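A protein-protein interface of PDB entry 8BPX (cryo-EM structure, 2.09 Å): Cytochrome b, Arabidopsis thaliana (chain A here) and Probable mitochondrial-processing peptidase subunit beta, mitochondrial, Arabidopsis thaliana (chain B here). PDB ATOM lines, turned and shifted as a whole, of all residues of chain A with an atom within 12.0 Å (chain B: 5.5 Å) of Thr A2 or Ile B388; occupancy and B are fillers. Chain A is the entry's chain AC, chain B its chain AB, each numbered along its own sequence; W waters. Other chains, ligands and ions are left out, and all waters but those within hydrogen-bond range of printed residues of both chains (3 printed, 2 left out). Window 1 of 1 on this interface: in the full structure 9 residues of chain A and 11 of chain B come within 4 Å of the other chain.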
ATOM      1  N   THR A   2      27.130 -21.058 -17.710  1.00  0.00           N
ATOM      2  CA  THR A   2      26.634 -19.858 -18.373  1.00  0.00           C
ATOM      3  C   THR A   2      25.112 -19.784 -18.306  1.00  0.00           C
ATOM      4  O   THR A   2      24.433 -20.809 -18.284  1.00  0.00           O
ATOM      5  CB  THR A   2      27.079 -19.803 -19.843  1.00  0.00           C
ATOM      6  OG1 THR A   2      26.275 -20.694 -20.624  1.00  0.00           O
ATOM      7  CG2 THR A   2      28.546 -20.198 -19.972  1.00  0.00           C
ATOM      8  N   ILE A   3      24.583 -18.566 -18.276  1.00  0.00           N
ATOM      9  CA  ILE A   3      23.147 -18.328 -18.189  1.00  0.00           C
ATOM     10  C   ILE A   3      22.631 -18.028 -19.588  1.00  0.00           C
ATOM     11  O   ILE A   3      23.117 -17.106 -20.252  1.00  0.00           O
ATOM     12  CB  ILE A   3      22.825 -17.181 -17.221  1.00  0.00           C
ATOM     13  CG1 ILE A   3      23.719 -17.264 -15.982  1.00  0.00           C
ATOM     14  CG2 ILE A   3      21.357 -17.212 -16.834  1.00  0.00           C
ATOM     15  CD1 ILE A   3      23.264 -16.392 -14.831  1.00  0.00           C
ATOM     16  N   ARG A   4      21.637 -18.796 -20.030  1.00  0.00           N
ATOM     17  CA  ARG A   4      21.149 -18.728 -21.409  1.00  0.00           C
ATOM     18  C   ARG A   4      20.013 -17.710 -21.520  1.00  0.00           C
ATOM     19  O   ARG A   4      18.858 -18.036 -21.798  1.00  0.00           O
ATOM     20  CB  ARG A   4      20.706 -20.109 -21.876  1.00  0.00           C
ATOM     21  CG  ARG A   4      21.841 -21.030 -22.263  1.00  0.00           C
ATOM     22  CD  ARG A   4      21.437 -22.487 -22.139  1.00  0.00           C
ATOM     23  NE  ARG A   4      22.509 -23.307 -21.591  1.00  0.00           N
ATOM     24  CZ  ARG A   4      23.589 -23.684 -22.264  1.00  0.00           C
ATOM     25  NH1 ARG A   4      23.771 -23.341 -23.529  1.00  0.00           N
ATOM     26  NH2 ARG A   4      24.508 -24.424 -21.653  1.00  0.00           N
ATOM     27  N   ASN A   5      20.370 -16.444 -21.304  1.00  0.00           N
ATOM     28  CA  ASN A   5      19.394 -15.371 -21.456  1.00  0.00           C
ATOM     29  C   ASN A   5      19.075 -15.102 -22.922  1.00  0.00           C
ATOM     30  O   ASN A   5      17.906 -14.943 -23.287  1.00  0.00           O
ATOM     31  CB  ASN A   5      19.903 -14.099 -20.783  1.00  0.00           C
ATOM     32  CG  ASN A   5      19.797 -14.161 -19.281  1.00  0.00           C
ATOM     33  OD1 ASN A   5      19.172 -15.064 -18.731  1.00  0.00           O
ATOM     34  ND2 ASN A   5      20.415 -13.203 -18.603  1.00  0.00           N
ATOM     35  N   GLN A   6      20.094 -15.044 -23.767  1.00  0.00           N
ATOM     36  CA  GLN A   6      19.925 -14.761 -25.184  1.00  0.00           C
ATOM     37  C   GLN A   6      20.003 -16.050 -25.993  1.00  0.00           C
ATOM     38  O   GLN A   6      20.338 -17.120 -25.482  1.00  0.00           O
ATOM     39  CB  GLN A   6      20.985 -13.765 -25.657  1.00  0.00           C
ATOM     40  CG  GLN A   6      21.191 -12.601 -24.710  1.00  0.00           C
ATOM     41  CD  GLN A   6      21.935 -11.449 -25.349  1.00  0.00           C
ATOM     42  OE1 GLN A   6      21.525 -10.297 -25.240  1.00  0.00           O
ATOM     43  NE2 GLN A   6      23.046 -11.756 -26.008  1.00  0.00           N
ATOM     44  N   ARG A   7      19.684 -15.934 -27.276  1.00  0.00           N
ATOM     45  CA  ARG A   7      19.796 -17.062 -28.186  1.00  0.00           C
ATOM     46  C   ARG A   7      21.170 -17.076 -28.849  1.00  0.00           C
ATOM     47  O   ARG A   7      21.602 -16.089 -29.451  1.00  0.00           O
ATOM     48  CB  ARG A   7      18.696 -17.011 -29.245  1.00  0.00           C
ATOM     49  CG  ARG A   7      17.290 -17.218 -28.692  1.00  0.00           C
ATOM     50  CD  ARG A   7      16.303 -17.575 -29.790  1.00  0.00           C
ATOM     51  NE  ARG A   7      16.169 -16.507 -30.769  1.00  0.00           N
ATOM     52  CZ  ARG A   7      15.120 -15.703 -30.870  1.00  0.00           C
ATOM     53  NH1 ARG A   7      14.064 -15.838 -30.083  1.00  0.00           N
ATOM     54  NH2 ARG A   7      15.130 -14.736 -31.780  1.00  0.00           N
ATOM     55  N   PHE A   8      21.859 -18.196 -28.703  1.00  0.00           N
ATOM     56  CA  PHE A   8      23.124 -18.469 -29.383  1.00  0.00           C
ATOM     57  C   PHE A   8      22.822 -19.217 -30.680  1.00  0.00           C
ATOM     58  O   PHE A   8      21.717 -19.052 -31.209  1.00  0.00           O
ATOM     59  CB  PHE A   8      24.077 -19.174 -28.428  1.00  0.00           C
ATOM     60  CG  PHE A   8      24.662 -18.264 -27.395  1.00  0.00           C
ATOM     61  CD1 PHE A   8      25.737 -17.447 -27.703  1.00  0.00           C
ATOM     62  CD2 PHE A   8      24.126 -18.208 -26.122  1.00  0.00           C
ATOM     63  CE1 PHE A   8      26.273 -16.599 -26.757  1.00  0.00           C
ATOM     64  CE2 PHE A   8      24.657 -17.361 -25.170  1.00  0.00           C
ATOM     65  CZ  PHE A   8      25.731 -16.554 -25.487  1.00  0.00           C
ATOM     66  N   SER A   9      23.754 -20.015 -31.190  1.00  0.00           N
ATOM     67  CA  SER A   9      23.468 -20.933 -32.325  1.00  0.00           C
ATOM     68  C   SER A   9      22.014 -21.444 -32.291  1.00  0.00           C
ATOM     69  O   SER A   9      21.585 -21.995 -31.274  1.00  0.00           O
ATOM     70  CB  SER A   9      24.441 -22.072 -32.366  1.00  0.00           C
ATOM     71  OG  SER A   9      24.179 -22.941 -33.450  1.00  0.00           O
ATOM     72  N   LYS A  12      21.519 -25.096 -31.069  1.00  0.00           N
ATOM     73  CA  LYS A  12      21.352 -25.352 -29.646  1.00  0.00           C
ATOM     74  C   LYS A  12      19.993 -24.909 -29.114  1.00  0.00           C
ATOM     75  O   LYS A  12      19.739 -25.049 -27.916  1.00  0.00           O
ATOM     76  CB  LYS A  12      22.475 -24.684 -28.848  1.00  0.00           C
ATOM     77  CG  LYS A  12      23.724 -25.545 -28.733  1.00  0.00           C
ATOM     78  CD  LYS A  12      24.983 -24.715 -28.621  1.00  0.00           C
ATOM     79  CE  LYS A  12      25.583 -24.809 -27.227  1.00  0.00           C
ATOM     80  NZ  LYS A  12      26.916 -24.146 -27.144  1.00  0.00           N
ATOM     81  N   GLN A  13      19.121 -24.380 -29.967  1.00  0.00           N
ATOM     82  CA  GLN A  13      17.771 -24.052 -29.542  1.00  0.00           C
ATOM     83  C   GLN A  13      16.938 -25.327 -29.411  1.00  0.00           C
ATOM     84  O   GLN A  13      17.264 -26.353 -30.016  1.00  0.00           O
ATOM     85  CB  GLN A  13      17.121 -23.091 -30.533  1.00  0.00           C
ATOM     86  CG  GLN A  13      17.565 -21.652 -30.361  1.00  0.00           C
ATOM     87  CD  GLN A  13      17.365 -21.137 -28.948  1.00  0.00           C
ATOM     88  OE1 GLN A  13      18.312 -20.709 -28.291  1.00  0.00           O
ATOM     89  NE2 GLN A  13      16.123 -21.150 -28.486  1.00  0.00           N
ATOM     90  N   ARG B 382      26.766  -9.212 -25.145  1.00  0.00           N
ATOM     91  CA  ARG B 382      26.477 -10.642 -25.114  1.00  0.00           C
ATOM     92  C   ARG B 382      27.225 -11.323 -23.974  1.00  0.00           C
ATOM     93  O   ARG B 382      26.640 -12.090 -23.192  1.00  0.00           O
ATOM     94  CB  ARG B 382      26.841 -11.269 -26.460  1.00  0.00           C
ATOM     95  CG  ARG B 382      25.719 -11.242 -27.478  1.00  0.00           C
ATOM     96  CD  ARG B 382      26.201 -11.617 -28.867  1.00  0.00           C
ATOM     97  NE  ARG B 382      25.428 -10.972 -29.921  1.00  0.00           N
ATOM     98  CZ  ARG B 382      24.178 -11.285 -30.242  1.00  0.00           C
ATOM     99  NH1 ARG B 382      23.519 -12.239 -29.606  1.00  0.00           N
ATOM    100  NH2 ARG B 382      23.575 -10.623 -31.223  1.00  0.00           N
ATOM    101  N   VAL B 383      28.514 -11.003 -23.832  1.00  0.00           N
ATOM    102  CA  VAL B 383      29.338 -11.647 -22.813  1.00  0.00           C
ATOM    103  C   VAL B 383      28.838 -11.298 -21.415  1.00  0.00           C
ATOM    104  O   VAL B 383      28.702 -12.172 -20.554  1.00  0.00           O
ATOM    105  CB  VAL B 383      30.817 -11.263 -23.004  1.00  0.00           C
ATOM    106  CG1 VAL B 383      31.632 -11.644 -21.782  1.00  0.00           C
ATOM    107  CG2 VAL B 383      31.369 -11.925 -24.255  1.00  0.00           C
ATOM    108  N   ASN B 386      25.134 -12.759 -20.645  1.00  0.00           N
ATOM    109  CA  ASN B 386      25.010 -14.195 -20.435  1.00  0.00           C
ATOM    110  C   ASN B 386      26.081 -14.788 -19.519  1.00  0.00           C
ATOM    111  O   ASN B 386      26.067 -16.001 -19.294  1.00  0.00           O
ATOM    112  CB  ASN B 386      24.997 -14.915 -21.782  1.00  0.00           C
ATOM    113  CG  ASN B 386      23.884 -14.419 -22.685  1.00  0.00           C
ATOM    114  OD1 ASN B 386      22.787 -14.967 -22.687  1.00  0.00           O
ATOM    115  ND2 ASN B 386      24.162 -13.382 -23.460  1.00  0.00           N
ATOM    116  N   GLU B 387      26.972 -13.971 -18.960  1.00  0.00           N
ATOM    117  CA  GLU B 387      28.033 -14.426 -18.054  1.00  0.00           C
ATOM    118  C   GLU B 387      28.825 -15.588 -18.660  1.00  0.00           C
ATOM    119  O   GLU B 387      28.853 -16.698 -18.132  1.00  0.00           O
ATOM    120  CB  GLU B 387      27.473 -14.827 -16.684  1.00  0.00           C
ATOM    121  CG  GLU B 387      26.722 -13.749 -15.918  1.00  0.00           C
ATOM    122  CD  GLU B 387      25.320 -13.517 -16.443  1.00  0.00           C
ATOM    123  OE1 GLU B 387      25.053 -12.406 -16.943  1.00  0.00           O
ATOM    124  OE2 GLU B 387      24.487 -14.445 -16.360  1.00  0.00           O
ATOM    125  N   ILE B 388      29.472 -15.319 -19.788  1.00  0.00           N
ATOM    126  CA  ILE B 388      30.131 -16.387 -20.526  1.00  0.00           C
ATOM    127  C   ILE B 388      31.638 -16.161 -20.639  1.00  0.00           C
ATOM    128  O   ILE B 388      32.291 -16.776 -21.469  1.00  0.00           O
ATOM    129  CB  ILE B 388      29.489 -16.579 -21.912  1.00  0.00           C
ATOM    130  CG1 ILE B 388      29.499 -15.267 -22.697  1.00  0.00           C
ATOM    131  CG2 ILE B 388      28.077 -17.122 -21.774  1.00  0.00           C
ATOM    132  CD1 ILE B 388      29.045 -15.414 -24.126  1.00  0.00           C
ATOM    133  N   ALA B 389      32.198 -15.285 -19.809  1.00  0.00           N
ATOM    134  CA  ALA B 389      33.637 -15.060 -19.805  1.00  0.00           C
ATOM    135  C   ALA B 389      34.036 -14.366 -18.512  1.00  0.00           C
ATOM    136  O   ALA B 389      33.220 -13.700 -17.873  1.00  0.00           O
ATOM    137  CB  ALA B 389      34.088 -14.224 -21.009  1.00  0.00           C
ATOM    138  N   GLU B 390      35.301 -14.545 -18.134  1.00  0.00           N
ATOM    139  CA  GLU B 390      35.889 -13.728 -17.078  1.00  0.00           C
ATOM    140  C   GLU B 390      36.382 -12.396 -17.616  1.00  0.00           C
ATOM    141  O   GLU B 390      36.295 -11.377 -16.924  1.00  0.00           O
ATOM    142  CB  GLU B 390      37.050 -14.465 -16.412  1.00  0.00           C
ATOM    143  CG  GLU B 390      36.740 -15.879 -16.001  1.00  0.00           C
ATOM    144  CD  GLU B 390      35.859 -15.938 -14.779  1.00  0.00           C
ATOM    145  OE1 GLU B 390      36.388 -15.759 -13.664  1.00  0.00           O
ATOM    146  OE2 GLU B 390      34.641 -16.160 -14.933  1.00  0.00           O
ATOM    147  N   VAL B 410      39.270 -14.863 -21.557  1.00  0.00           N
ATOM    148  CA  VAL B 410      39.469 -15.770 -20.432  1.00  0.00           C
ATOM    149  C   VAL B 410      38.094 -16.226 -19.962  1.00  0.00           C
ATOM    150  O   VAL B 410      37.210 -15.393 -19.729  1.00  0.00           O
ATOM    151  CB  VAL B 410      40.245 -15.093 -19.283  1.00  0.00           C
ATOM    152  CG1 VAL B 410      40.468 -16.059 -18.136  1.00  0.00           C
ATOM    153  CG2 VAL B 410      41.562 -14.527 -19.783  1.00  0.00           C
ATOM    154  N   ALA B 411      37.907 -17.538 -19.828  1.00  0.00           N
ATOM    155  CA  ALA B 411      36.601 -18.074 -19.465  1.00  0.00           C
ATOM    156  C   ALA B 411      36.762 -19.466 -18.870  1.00  0.00           C
ATOM    157  O   ALA B 411      37.812 -20.099 -18.988  1.00  0.00           O
ATOM    158  CB  ALA B 411      35.657 -18.117 -20.669  1.00  0.00           C
ATOM    159  N   ASP B 414      33.198 -24.653 -19.504  1.00  0.00           N
ATOM    160  CA  ASP B 414      31.854 -24.886 -20.007  1.00  0.00           C
ATOM    161  C   ASP B 414      31.254 -23.683 -20.723  1.00  0.00           C
ATOM    162  O   ASP B 414      30.184 -23.816 -21.322  1.00  0.00           O
ATOM    163  CB  ASP B 414      30.941 -25.317 -18.861  1.00  0.00           C
ATOM    164  CG  ASP B 414      31.295 -26.686 -18.329  1.00  0.00           C
ATOM    165  OD1 ASP B 414      31.749 -27.530 -19.128  1.00  0.00           O
ATOM    166  OD2 ASP B 414      31.128 -26.918 -17.112  1.00  0.00           O
ATOM    167  N   CYS B 415      31.902 -22.525 -20.681  1.00  0.00           N
ATOM    168  CA  CYS B 415      31.417 -21.356 -21.400  1.00  0.00           C
ATOM    169  C   CYS B 415      32.022 -21.217 -22.791  1.00  0.00           C
ATOM    170  O   CYS B 415      31.548 -20.378 -23.569  1.00  0.00           O
ATOM    171  CB  CYS B 415      31.702 -20.088 -20.589  1.00  0.00           C
ATOM    172  SG  CYS B 415      31.245 -20.199 -18.841  1.00  0.00           S
ATOM    173  N   ASP B 418      29.803 -21.261 -26.319  1.00  0.00           N
ATOM    174  CA  ASP B 418      28.994 -20.062 -26.512  1.00  0.00           C
ATOM    175  C   ASP B 418      29.862 -18.824 -26.684  1.00  0.00           C
ATOM    176  O   ASP B 418      29.543 -17.946 -27.494  1.00  0.00           O
ATOM    177  CB  ASP B 418      28.024 -19.882 -25.345  1.00  0.00           C
ATOM    178  CG  ASP B 418      26.880 -20.875 -25.382  1.00  0.00           C
ATOM    179  OD1 ASP B 418      26.306 -21.079 -26.470  1.00  0.00           O
ATOM    180  OD2 ASP B 418      26.543 -21.441 -24.321  1.00  0.00           O
ATOM    181  N   LEU B 419      30.963 -18.732 -25.934  1.00  0.00           N
ATOM    182  CA  LEU B 419      31.848 -17.582 -26.066  1.00  0.00           C
ATOM    183  C   LEU B 419      32.445 -17.505 -27.465  1.00  0.00           C
ATOM    184  O   LEU B 419      32.504 -16.427 -28.067  1.00  0.00           O
ATOM    185  CB  LEU B 419      32.951 -17.650 -25.014  1.00  0.00           C
ATOM    186  CG  LEU B 419      33.922 -16.473 -24.993  1.00  0.00           C
ATOM    187  CD1 LEU B 419      33.177 -15.163 -24.805  1.00  0.00           C
ATOM    188  CD2 LEU B 419      34.967 -16.670 -23.914  1.00  0.00           C
ATOM    189  N   ALA B 422      29.863 -16.346 -29.914  1.00  0.00           N
ATOM    190  CA  ALA B 422      29.592 -14.914 -29.801  1.00  0.00           C
ATOM    191  C   ALA B 422      30.713 -14.080 -30.409  1.00  0.00           C
ATOM    192  O   ALA B 422      30.454 -13.111 -31.136  1.00  0.00           O
ATOM    193  CB  ALA B 422      29.380 -14.530 -28.337  1.00  0.00           C
HETATM  194  O   HOH W   1      28.139 -23.234 -19.346  1.00  0.00           O
HETATM  195  O   HOH W   2      24.011 -13.976 -27.765  1.00  0.00           O
HETATM  196  O   HOH W   3      26.167 -21.210 -29.500  1.00  0.00           O
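Among the printed residues, pairs that only touch across the chains: Ile A3 with Glu B387 (2.8 Å), Thr A2 with Cys B415 (2.9 Å), Gln A6 with Arg B382 (3.1 Å), Phe A8 with Asp B418 (3.4 Å), Thr A2 with Ile B388 (3.5 Å), Phe A8 with Ile B388 (3.8 Å), Thr A2 with Asp B418 (3.8 Å), Thr A2 with Glu B387 (3.9 Å), Phe A8 with Asn B386 (3.9 Å) and Thr A2 with Asn B386 (3.97 Å).
Thr A2 touches just these residues of chain B: Asn B386, Glu B387, Ile B388, Cys B415 and Asp B418.
Of the printed residues of chain B, Ile A3 touches Asn B386 (3.1 Å) and Glu B387 (2.8 Å).
Of the printed residues of chain B, Arg A4 touches Asp B418 (3.5 Å).
Printed residues of chain B within 4 Å of Asn A5: Asn B386.
Of the printed residues of chain B, Gln A6 touches Arg B382 (3.1 Å) and Asn B386 (2.9 Å).
Printed residues of chain B within 4 Å of Phe A8: Asn B386, Ile B388 and Asp B418.
Gln A13 touches none of the printed residues of chain B.
Of chain A, only Thr A2, Ile A3, Asn A5, Gln A6 and Phe A8 come within 4 Å of Asn B386.
Glu B387 touches just these residues of chain A: Thr A2 (3.9 Å) and Ile A3 (2.8 Å).
Of chain A, only Thr A2 (3.5 Å) and Phe A8 (3.8 Å) come within 4 Å of Ile B388.
No residue of chain A comes within 4 Å of Ala B389.
Val B410 touches none of the printed residues of chain A.
No residue of chain A comes within 4 Å of Ala B411.
Cys B415 touches just one residue of chain A: Thr A2 (2.9 Å).
No residue of chain A comes within 4 Å of Leu B419.
No residue of chain A comes within 4 Å of Ala B422.
The nearest residue of chain B that does not touch Thr A2 is Asp B414 (4.2 Å).
The nearest printed residue of chain B that does not touch Asn A5 is Glu B387 (4.8 Å).
O of Asn B386 sits at hydrogen-bond distance from N of Ile A3.
N of Asn A5 lies within hydrogen-bond range of OD1 of Asn B386 (3.2 Å).
OD1 of Asn B386 lies within hydrogen-bond range of N of Gln A6, at 2.9 Å.
The guanidinium group (NH1) of Arg A4 is in salt-bridge range of the side-chain carboxylate (OD2) of Asp B418.
The side-chain amino group (NZ) of Lys A12 lies within salt-bridge range of the side-chain carboxylate (OD1) of Asp B418, 3.2 Å away.
Hydrophobic or aromatic side chains of chain A that line the printed part of chain B: Ile A3 and Phe A8.
Hydrophobic or aromatic side chains of chain B that line the printed part of chain A: Ile B388.
Among the printed residues, 15 pairs touch across the chains.
Among the printed residues, Asp or Glu carboxylates within 4 Å of a Lys or Arg side-chain nitrogen of the other chain: Arg A4 with Asp B418 and Lys A12 with Asp B418.
The backbone carbonyl oxygen of Arg B382 is in hydrogen-bond range of the side-chain amide nitrogen of Asn B386 (2.8 Å).
The backbone NH (N) of Ile B388 lies within hydrogen-bond range of the backbone carbonyl oxygen (O) of Val B383 (3.3 Å).
Water W2 lies within hydrogen-bond range of NH1 of Arg B382 (2.6 Å) and NE2 of Gln A6 (3.0 Å).
Water W1 bridges the backbone carbonyl oxygen of Asp B414 (2.9 Å) and the backbone NH of Thr A2 (2.9 Å).
Water W3 lies within hydrogen-bond range of the side-chain carboxylate (OD1) of Asp B418 (3.0 Å) and the backbone NH (N) of Ser A9 (3.2 Å).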
